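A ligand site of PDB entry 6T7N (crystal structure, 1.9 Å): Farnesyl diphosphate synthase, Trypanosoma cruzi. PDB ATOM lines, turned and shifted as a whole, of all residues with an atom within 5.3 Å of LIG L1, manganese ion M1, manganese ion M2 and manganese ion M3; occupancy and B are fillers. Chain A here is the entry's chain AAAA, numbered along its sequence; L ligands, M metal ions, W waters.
Manganese ion M3 is bound by water W2 (1.9 Å), O3 of LIG L1 (2.0 Å), OD1 of Asp 98 (2.1 Å), water W3 (2.1 Å), OD2 of Asp 102 (2.2 Å) and water W4 (2.2 Å).
Manganese ion M3 has six donor atoms within binding distance.
Merely in contact with manganese ion M2: Asp 254 (3.8 Å).
Of the 21 residues printed, 2 come within 4 Å of manganese ion M2.
Along chain A the residues within 4 Å of manganese ion M2 span positions 250 to 254.
The nearest printed residue that does not touch manganese ion M2 is Lys 264 (4.1 Å).
Water W9 bridges the side-chain hydroxyl (OG) of Ser 104 (2.7 Å) and the side-chain carboxylate (OD1) of Asp 99 (2.9 Å).
Water W7 bridges the side-chain carboxylate (OD2) of Asp 254 (2.9 Å) and the backbone carbonyl oxygen (O) of Asp 250 (3.0 Å).
Water W6 lies within hydrogen-bond range of OD2 of Asp 268 (2.5 Å), OD1 of Asp 251 (2.7 Å) and O2 of LIG L1 (3.4 Å).
Water W4 lies within hydrogen-bond range of the side-chain amino group of Lys 273 (2.6 Å) and the side-chain carboxylate of Asp 170 (2.7 Å).
Water W2 lies within hydrogen-bond range of the side-chain carboxylate of Asp 102 (2.4 Å) and the side-chain carboxylate of Asp 170 (2.8 Å).
Water W1 lies within hydrogen-bond range of an oxygen (O2) of LIG L1 (2.7 Å), the side-chain carboxylate (OD1) of Asp 268 (3.0 Å) and the side-chain amino group (NZ) of Lys 207 (3.3 Å).
CG2 of Thr 163 touches C5 of LIG L1, 3.97 Å away.
Gln 167 touches LIG L1 (CD to C5, 3.6 Å).
OG1 of Thr 208 touches C2 of LIG L1, at 3.8 Å.
Tyr 211 touches LIG L1.
Gln 247 touches LIG L1 (NE2 to O2, 3.6 Å).
11 residues have an atom within 4 Å of LIG L1: Asp 98, Asp 102, Arg 107, Thr 163, Gln 167, Lys 207, Thr 208, Tyr 211, Gln 247, Asp 250 and Lys 264.
Manganese ion M2 is bound by an oxygen (O6) of LIG L1 (1.9 Å), the side-chain carboxylate of Asp 250 (2.0 Å), water W7 (2.1 Å), water W6 (2.2 Å) and water W8 (2.4 Å).
Manganese ion M2 has five donor atoms within binding distance.
Slightly farther from manganese ion M2 lies an oxygen (O2) of LIG L1 (2.9 Å).
OD2 of Asp 170 touches manganese ion M3 (3.6 Å).
Within 4 Å of manganese ion M3: Asp 98, Asp 102 and Asp 170.
The side-chain amino group (NZ) of Lys 264 is in salt-bridge range of an oxygen (O7) of LIG L1, at 2.7 Å.
NZ of Lys 207 lies within salt-bridge range of O2 of LIG L1 (3.3 Å).
O7 of LIG L1 is in salt-bridge range of NH1 of Arg 107 (2.8 Å).
Within 4 Å of manganese ion M1: Asp 98 and Asp 102.
The nearest printed residue that does not touch manganese ion M1 is Arg 107 (4.2 Å).
Manganese ion M1 is bound by the side-chain carboxylate (OD2) of Asp 98 (2.0 Å), water W9 (2.0 Å), an oxygen (O5) of LIG L1 (2.0 Å), water W5 (2.1 Å), the side-chain carboxylate (OD2) of Asp 102 (2.1 Å) and an oxygen (O3) of LIG L1 (2.3 Å).
OG1 of Thr 163 lies close to OH of Tyr 94, 3.4 Å away.
OD1 of Asp 254 sits at hydrogen-bond distance from N of Asp 268, at 3.2 Å.
The side-chain carboxylate (OD2) of Asp 250 lies close to the side-chain amide nitrogen (NE2) of Gln 247 (3.0 Å).
OD1 of Asp 170 is in salt-bridge range of NZ of Lys 207 (2.9 Å).
The side-chain carboxylate (OD2) of Asp 98 lies close to the guanidinium group (NH2) of Arg 107 (3.8 Å).
NE2 of Gln 167 sits close to OD1 of Asp 98, at 3.1 Å.
OD1 of Asp 250 is in salt-bridge range of NZ of Lys 264 (2.7 Å).
NE2 of Gln 247 is in hydrogen-bond range of OD1 of Asp 251.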
ATOM      1  N   TYR A  94     -17.825   5.193 -11.786  1.00  0.00           N
ATOM      2  CA  TYR A  94     -16.688   5.970 -11.268  1.00  0.00           C
ATOM      3  C   TYR A  94     -15.378   5.541 -11.922  1.00  0.00           C
ATOM      4  O   TYR A  94     -14.522   6.377 -12.216  1.00  0.00           O
ATOM      5  CB  TYR A  94     -16.568   5.812  -9.735  1.00  0.00           C
ATOM      6  CG  TYR A  94     -17.719   6.336  -8.929  1.00  0.00           C
ATOM      7  CD1 TYR A  94     -18.259   7.590  -9.168  1.00  0.00           C
ATOM      8  CD2 TYR A  94     -18.244   5.579  -7.888  1.00  0.00           C
ATOM      9  CE1 TYR A  94     -19.335   8.077  -8.395  1.00  0.00           C
ATOM     10  CE2 TYR A  94     -19.280   6.052  -7.103  1.00  0.00           C
ATOM     11  CZ  TYR A  94     -19.837   7.295  -7.379  1.00  0.00           C
ATOM     12  OH  TYR A  94     -20.868   7.755  -6.585  1.00  0.00           O
ATOM     13  N   LEU A  95     -15.184   4.228 -12.111  1.00  0.00           N
ATOM     14  CA  LEU A  95     -13.915   3.761 -12.676  1.00  0.00           C
ATOM     15  C   LEU A  95     -13.749   4.184 -14.127  1.00  0.00           C
ATOM     16  O   LEU A  95     -12.637   4.500 -14.569  1.00  0.00           O
ATOM     17  CB  LEU A  95     -13.809   2.238 -12.554  1.00  0.00           C
ATOM     18  CG  LEU A  95     -13.865   1.640 -11.148  1.00  0.00           C
ATOM     19  CD1 LEU A  95     -13.514   0.148 -11.150  1.00  0.00           C
ATOM     20  CD2 LEU A  95     -12.928   2.409 -10.214  1.00  0.00           C
ATOM     21  N   ASP A  98     -12.921   7.823 -13.825  1.00  0.00           N
ATOM     22  CA  ASP A  98     -11.664   7.997 -13.098  1.00  0.00           C
ATOM     23  C   ASP A  98     -10.464   7.630 -13.949  1.00  0.00           C
ATOM     24  O   ASP A  98      -9.408   8.290 -13.881  1.00  0.00           O
ATOM     25  CB  ASP A  98     -11.678   7.156 -11.819  1.00  0.00           C
ATOM     26  CG  ASP A  98     -10.383   7.282 -10.994  1.00  0.00           C
ATOM     27  OD1 ASP A  98     -10.268   8.267 -10.216  1.00  0.00           O
ATOM     28  OD2 ASP A  98      -9.520   6.386 -11.110  1.00  0.00           O
ATOM     29  N   ASP A  99     -10.571   6.551 -14.737  1.00  0.00           N
ATOM     30  CA  ASP A  99      -9.443   6.134 -15.561  1.00  0.00           C
ATOM     31  C   ASP A  99      -9.136   7.192 -16.616  1.00  0.00           C
ATOM     32  O   ASP A  99      -7.953   7.450 -16.909  1.00  0.00           O
ATOM     33  CB  ASP A  99      -9.725   4.786 -16.215  1.00  0.00           C
ATOM     34  CG  ASP A  99      -9.516   3.649 -15.260  1.00  0.00           C
ATOM     35  OD1 ASP A  99      -8.769   3.834 -14.277  1.00  0.00           O
ATOM     36  OD2 ASP A  99     -10.092   2.573 -15.460  1.00  0.00           O
ATOM     37  N   ASP A 102      -7.482  10.089 -14.594  1.00  0.00           N
ATOM     38  CA  ASP A 102      -6.170   9.803 -14.010  1.00  0.00           C
ATOM     39  C   ASP A 102      -5.133   9.422 -15.064  1.00  0.00           C
ATOM     40  O   ASP A 102      -3.944   9.222 -14.729  1.00  0.00           O
ATOM     41  CB  ASP A 102      -6.329   8.687 -12.962  1.00  0.00           C
ATOM     42  CG  ASP A 102      -7.116   9.124 -11.751  1.00  0.00           C
ATOM     43  OD1 ASP A 102      -7.438  10.326 -11.649  1.00  0.00           O
ATOM     44  OD2 ASP A 102      -7.411   8.256 -10.897  1.00  0.00           O
ATOM     45  N   SER A 104      -5.042   6.582 -16.879  1.00  0.00           N
ATOM     46  CA  SER A 104      -4.606   5.215 -16.611  1.00  0.00           C
ATOM     47  C   SER A 104      -4.691   4.361 -17.872  1.00  0.00           C
ATOM     48  O   SER A 104      -5.368   4.723 -18.835  1.00  0.00           O
ATOM     49  CB  SER A 104      -5.457   4.641 -15.482  1.00  0.00           C
ATOM     50  OG  SER A 104      -5.283   5.438 -14.310  1.00  0.00           O
ATOM     51  N   ARG A 107      -7.123  -1.681 -16.334  1.00  0.00           N
ATOM     52  CA  ARG A 107      -8.142  -1.845 -15.308  1.00  0.00           C
ATOM     53  C   ARG A 107      -8.598  -3.292 -15.330  1.00  0.00           C
ATOM     54  O   ARG A 107      -8.990  -3.796 -16.397  1.00  0.00           O
ATOM     55  CB  ARG A 107      -9.327  -0.884 -15.527  1.00  0.00           C
ATOM     56  CG  ARG A 107     -10.530  -1.095 -14.557  1.00  0.00           C
ATOM     57  CD  ARG A 107     -10.144  -0.699 -13.121  1.00  0.00           C
ATOM     58  NE  ARG A 107      -9.947   0.751 -12.991  1.00  0.00           N
ATOM     59  CZ  ARG A 107      -9.647   1.368 -11.851  1.00  0.00           C
ATOM     60  NH1 ARG A 107      -9.479   0.656 -10.735  1.00  0.00           N
ATOM     61  NH2 ARG A 107      -9.508   2.680 -11.840  1.00  0.00           N
ATOM     62  N   THR A 163     -19.226  11.188  -3.262  1.00  0.00           N
ATOM     63  CA  THR A 163     -18.130  10.641  -4.044  1.00  0.00           C
ATOM     64  C   THR A 163     -17.635  11.626  -5.095  1.00  0.00           C
ATOM     65  O   THR A 163     -16.426  11.762  -5.324  1.00  0.00           O
ATOM     66  CB  THR A 163     -18.566   9.337  -4.698  1.00  0.00           C
ATOM     67  OG1 THR A 163     -19.110   8.469  -3.708  1.00  0.00           O
ATOM     68  CG2 THR A 163     -17.416   8.671  -5.374  1.00  0.00           C
ATOM     69  N   GLN A 167     -14.013  13.236  -5.526  1.00  0.00           N
ATOM     70  CA  GLN A 167     -13.224  13.219  -6.747  1.00  0.00           C
ATOM     71  C   GLN A 167     -12.700  14.617  -7.074  1.00  0.00           C
ATOM     72  O   GLN A 167     -11.586  14.760  -7.600  1.00  0.00           O
ATOM     73  CB  GLN A 167     -14.049  12.642  -7.899  1.00  0.00           C
ATOM     74  CG  GLN A 167     -14.152  11.141  -7.858  1.00  0.00           C
ATOM     75  CD  GLN A 167     -12.837  10.437  -8.161  1.00  0.00           C
ATOM     76  OE1 GLN A 167     -11.890  10.492  -7.368  1.00  0.00           O
ATOM     77  NE2 GLN A 167     -12.773   9.794  -9.319  1.00  0.00           N
ATOM     78  N   ASP A 170      -9.818  15.017  -4.861  1.00  0.00           N
ATOM     79  CA  ASP A 170      -8.707  14.202  -5.357  1.00  0.00           C
ATOM     80  C   ASP A 170      -8.006  14.848  -6.550  1.00  0.00           C
ATOM     81  O   ASP A 170      -6.773  14.993  -6.556  1.00  0.00           O
ATOM     82  CB  ASP A 170      -9.221  12.801  -5.703  1.00  0.00           C
ATOM     83  CG  ASP A 170      -8.135  11.899  -6.224  1.00  0.00           C
ATOM     84  OD1 ASP A 170      -7.506  11.202  -5.418  1.00  0.00           O
ATOM     85  OD2 ASP A 170      -7.894  11.915  -7.453  1.00  0.00           O
ATOM     86  N   LYS A 207     -14.172  10.490  -1.371  1.00  0.00           N
ATOM     87  CA  LYS A 207     -14.064   9.801  -2.662  1.00  0.00           C
ATOM     88  C   LYS A 207     -14.292   8.309  -2.541  1.00  0.00           C
ATOM     89  O   LYS A 207     -14.664   7.676  -3.540  1.00  0.00           O
ATOM     90  CB  LYS A 207     -12.699  10.057  -3.346  1.00  0.00           C
ATOM     91  CG  LYS A 207     -11.516   9.234  -2.851  1.00  0.00           C
ATOM     92  CD  LYS A 207     -10.374   9.314  -3.866  1.00  0.00           C
ATOM     93  CE  LYS A 207      -9.123   8.571  -3.385  1.00  0.00           C
ATOM     94  NZ  LYS A 207      -7.990   8.581  -4.401  1.00  0.00           N
ATOM     95  N   THR A 208     -14.029   7.720  -1.366  1.00  0.00           N
ATOM     96  CA  THR A 208     -14.018   6.272  -1.247  1.00  0.00           C
ATOM     97  C   THR A 208     -14.985   5.715  -0.212  1.00  0.00           C
ATOM     98  O   THR A 208     -15.717   4.771  -0.513  1.00  0.00           O
ATOM     99  CB  THR A 208     -12.591   5.787  -0.936  1.00  0.00           C
ATOM    100  OG1 THR A 208     -11.764   6.085  -2.063  1.00  0.00           O
ATOM    101  CG2 THR A 208     -12.557   4.273  -0.637  1.00  0.00           C
ATOM    102  N   TYR A 211     -19.187   5.288  -0.681  1.00  0.00           N
ATOM    103  CA  TYR A 211     -19.741   4.360  -1.658  1.00  0.00           C
ATOM    104  C   TYR A 211     -19.160   2.971  -1.529  1.00  0.00           C
ATOM    105  O   TYR A 211     -19.815   2.000  -1.914  1.00  0.00           O
ATOM    106  CB  TYR A 211     -19.554   4.875  -3.105  1.00  0.00           C
ATOM    107  CG  TYR A 211     -18.308   4.461  -3.850  1.00  0.00           C
ATOM    108  CD1 TYR A 211     -17.132   5.180  -3.710  1.00  0.00           C
ATOM    109  CD2 TYR A 211     -18.314   3.377  -4.703  1.00  0.00           C
ATOM    110  CE1 TYR A 211     -16.020   4.836  -4.387  1.00  0.00           C
ATOM    111  CE2 TYR A 211     -17.186   2.996  -5.387  1.00  0.00           C
ATOM    112  CZ  TYR A 211     -16.037   3.745  -5.244  1.00  0.00           C
ATOM    113  OH  TYR A 211     -14.890   3.398  -5.943  1.00  0.00           O
ATOM    114  N   GLN A 247      -8.405   2.498   1.348  1.00  0.00           N
ATOM    115  CA  GLN A 247      -7.735   3.386   0.406  1.00  0.00           C
ATOM    116  C   GLN A 247      -6.223   3.447   0.668  1.00  0.00           C
ATOM    117  O   GLN A 247      -5.432   3.531  -0.277  1.00  0.00           O
ATOM    118  CB  GLN A 247      -8.360   4.771   0.473  1.00  0.00           C
ATOM    119  CG  GLN A 247      -7.787   5.687  -0.587  1.00  0.00           C
ATOM    120  CD  GLN A 247      -8.154   5.229  -1.995  1.00  0.00           C
ATOM    121  OE1 GLN A 247      -9.336   4.984  -2.300  1.00  0.00           O
ATOM    122  NE2 GLN A 247      -7.140   5.100  -2.840  1.00  0.00           N
ATOM    123  N   ASP A 250      -4.859   0.664  -1.088  1.00  0.00           N
ATOM    124  CA  ASP A 250      -4.864   0.905  -2.522  1.00  0.00           C
ATOM    125  C   ASP A 250      -3.715   1.829  -2.928  1.00  0.00           C
ATOM    126  O   ASP A 250      -3.098   1.653  -3.991  1.00  0.00           O
ATOM    127  CB  ASP A 250      -6.212   1.511  -2.930  1.00  0.00           C
ATOM    128  CG  ASP A 250      -6.276   1.815  -4.402  1.00  0.00           C
ATOM    129  OD1 ASP A 250      -6.385   0.831  -5.172  1.00  0.00           O
ATOM    130  OD2 ASP A 250      -6.204   3.009  -4.780  1.00  0.00           O
ATOM    131  N   ASP A 251      -3.425   2.812  -2.084  1.00  0.00           N
ATOM    132  CA  ASP A 251      -2.340   3.723  -2.377  1.00  0.00           C
ATOM    133  C   ASP A 251      -1.004   2.986  -2.321  1.00  0.00           C
ATOM    134  O   ASP A 251      -0.142   3.183  -3.188  1.00  0.00           O
ATOM    135  CB  ASP A 251      -2.326   4.887  -1.380  1.00  0.00           C
ATOM    136  CG  ASP A 251      -3.439   5.884  -1.624  1.00  0.00           C
ATOM    137  OD1 ASP A 251      -4.243   5.734  -2.573  1.00  0.00           O
ATOM    138  OD2 ASP A 251      -3.470   6.848  -0.834  1.00  0.00           O
ATOM    139  N   ASP A 254      -0.676   0.785  -5.410  1.00  0.00           N
ATOM    140  CA  ASP A 254      -0.454   1.581  -6.616  1.00  0.00           C
ATOM    141  C   ASP A 254       1.030   1.639  -6.968  1.00  0.00           C
ATOM    142  O   ASP A 254       1.410   1.569  -8.148  1.00  0.00           O
ATOM    143  CB  ASP A 254      -0.996   3.012  -6.415  1.00  0.00           C
ATOM    144  CG  ASP A 254      -0.998   3.888  -7.710  1.00  0.00           C
ATOM    145  OD1 ASP A 254       0.014   4.564  -8.033  1.00  0.00           O
ATOM    146  OD2 ASP A 254      -2.062   3.915  -8.398  1.00  0.00           O
ATOM    147  N   LYS A 264      -3.921  -3.252 -12.540  1.00  0.00           N
ATOM    148  CA  LYS A 264      -3.894  -1.890 -13.033  1.00  0.00           C
ATOM    149  C   LYS A 264      -2.468  -1.379 -12.858  1.00  0.00           C
ATOM    150  O   LYS A 264      -1.692  -1.945 -12.086  1.00  0.00           O
ATOM    151  CB  LYS A 264      -4.909  -0.996 -12.295  1.00  0.00           C
ATOM    152  CG  LYS A 264      -4.745  -0.967 -10.794  1.00  0.00           C
ATOM    153  CD  LYS A 264      -5.915  -0.214 -10.112  1.00  0.00           C
ATOM    154  CE  LYS A 264      -5.606   0.047  -8.639  1.00  0.00           C
ATOM    155  NZ  LYS A 264      -6.815   0.318  -7.823  1.00  0.00           N
ATOM    156  N   THR A 267      -0.701   5.359 -11.222  1.00  0.00           N
ATOM    157  CA  THR A 267      -0.401   6.671 -11.780  1.00  0.00           C
ATOM    158  C   THR A 267      -0.220   7.762 -10.718  1.00  0.00           C
ATOM    159  O   THR A 267      -0.081   8.934 -11.078  1.00  0.00           O
ATOM    160  CB  THR A 267      -1.508   7.125 -12.748  1.00  0.00           C
ATOM    161  OG1 THR A 267      -2.782   7.064 -12.066  1.00  0.00           O
ATOM    162  CG2 THR A 267      -1.508   6.256 -13.978  1.00  0.00           C
ATOM    163  N   ASP A 268      -0.236   7.407  -9.429  1.00  0.00           N
ATOM    164  CA  ASP A 268      -0.313   8.417  -8.374  1.00  0.00           C
ATOM    165  C   ASP A 268       0.918   9.327  -8.356  1.00  0.00           C
ATOM    166  O   ASP A 268       0.800  10.537  -8.160  1.00  0.00           O
ATOM    167  CB  ASP A 268      -0.479   7.757  -7.012  1.00  0.00           C
ATOM    168  CG  ASP A 268      -1.836   7.140  -6.818  1.00  0.00           C
ATOM    169  OD1 ASP A 268      -2.739   7.387  -7.638  1.00  0.00           O
ATOM    170  OD2 ASP A 268      -2.005   6.366  -5.838  1.00  0.00           O
ATOM    171  N   LYS A 273      -0.523  12.867  -7.062  1.00  0.00           N
ATOM    172  CA  LYS A 273      -1.624  12.696  -6.138  1.00  0.00           C
ATOM    173  C   LYS A 273      -1.182  12.800  -4.678  1.00  0.00           C
ATOM    174  O   LYS A 273      -0.046  12.470  -4.311  1.00  0.00           O
ATOM    175  CB  LYS A 273      -2.303  11.345  -6.358  1.00  0.00           C
ATOM    176  CG  LYS A 273      -3.032  11.236  -7.739  1.00  0.00           C
ATOM    177  CD  LYS A 273      -4.241  12.237  -7.803  1.00  0.00           C
ATOM    178  CE  LYS A 273      -4.828  12.393  -9.236  1.00  0.00           C
ATOM    179  NZ  LYS A 273      -5.309  11.103  -9.779  1.00  0.00           N
HETATM  180  C1  LIG L   1     -10.631   5.684  -5.895  1.00  0.00           C
HETATM  181  O1  LIG L   1      -9.657   6.506  -6.598  1.00  0.00           O
HETATM  182  C2  LIG L   1     -11.926   6.457  -5.801  1.00  0.00           C
HETATM  183  C3  LIG L   1     -12.781   6.518  -7.055  1.00  0.00           C
HETATM  184  C4  LIG L   1     -12.439   5.913  -8.193  1.00  0.00           C
HETATM  185  C5  LIG L   1     -14.038   7.293  -6.927  1.00  0.00           C
HETATM  186  P1  LIG L   1      -8.358   5.989  -7.345  1.00  0.00           P
HETATM  187  O2  LIG L   1      -7.256   5.995  -6.339  1.00  0.00           O
HETATM  188  O3  LIG L   1      -8.215   6.935  -8.584  1.00  0.00           O
HETATM  189  O4  LIG L   1      -8.691   4.543  -7.876  1.00  0.00           O
HETATM  190  P2  LIG L   1      -7.755   3.570  -8.724  1.00  0.00           P
HETATM  191  O5  LIG L   1      -7.625   4.269 -10.018  1.00  0.00           O
HETATM  192  O6  LIG L   1      -6.461   3.495  -7.918  1.00  0.00           O
HETATM  193  O7  LIG L   1      -8.450   2.237  -8.720  1.00  0.00           O
HETATM  194  C1  LG2 L   2     -10.929   0.609  -6.974  1.00  0.00           C
HETATM  195  O1  LG2 L   2     -11.803  -0.215  -6.180  1.00  0.00           O
HETATM  196  C2  LG2 L   2     -11.227   2.052  -6.681  1.00  0.00           C
HETATM  197  C3  LG2 L   2     -10.876   2.524  -5.275  1.00  0.00           C
HETATM  198  C4  LG2 L   2     -11.832   3.001  -4.483  1.00  0.00           C
HETATM  199  C5  LG2 L   2      -9.455   2.438  -4.836  1.00  0.00           C
HETATM  200  P1  LG2 L   2     -11.662  -1.790  -5.993  1.00  0.00           P
HETATM  201  O2  LG2 L   2     -10.201  -2.109  -5.645  1.00  0.00           O
HETATM  202  O3  LG2 L   2     -12.647  -2.344  -5.066  1.00  0.00           O
HETATM  203  O4  LG2 L   2     -11.889  -2.306  -7.487  1.00  0.00           O
HETATM  204  P2  LG2 L   2     -12.680  -3.568  -8.046  1.00  0.00           P
HETATM  205  O5  LG2 L   2     -14.116  -3.178  -8.261  1.00  0.00           O
HETATM  206  O6  LG2 L   2     -12.502  -4.723  -7.070  1.00  0.00           O
HETATM  207  O7  LG2 L   2     -11.981  -3.906  -9.375  1.00  0.00           O
HETATM  208 MN    MN M   1      -7.585   6.170 -10.646  1.00  0.00          MN
HETATM  209 MN    MN M   2      -5.345   3.870  -6.401  1.00  0.00          MN
HETATM  210 MN    MN M   3      -8.599   8.834  -9.165  1.00  0.00          MN
HETATM  211  O   HOH W   1      -5.504   7.996  -6.527  1.00  0.00           O
HETATM  212  O   HOH W   2      -8.950  10.604  -9.745  1.00  0.00           O
HETATM  213  O   HOH W   3      -9.848   9.070  -7.462  1.00  0.00           O
HETATM  214  O   HOH W   4      -6.794   9.624  -8.231  1.00  0.00           O
HETATM  215  O   HOH W   5      -5.544   6.257 -10.297  1.00  0.00           O
HETATM  216  O   HOH W   6      -4.133   5.250  -5.227  1.00  0.00           O
HETATM  217  O   HOH W   7      -3.940   2.353  -6.805  1.00  0.00           O
HETATM  218  O   HOH W   8      -4.200   5.164  -8.038  1.00  0.00           O
HETATM  219  O   HOH W   9      -7.283   5.625 -12.549  1.00  0.00           O
HETATM  220  O   HOH W  10      -5.546   2.911 -11.381  1.00  0.00           O
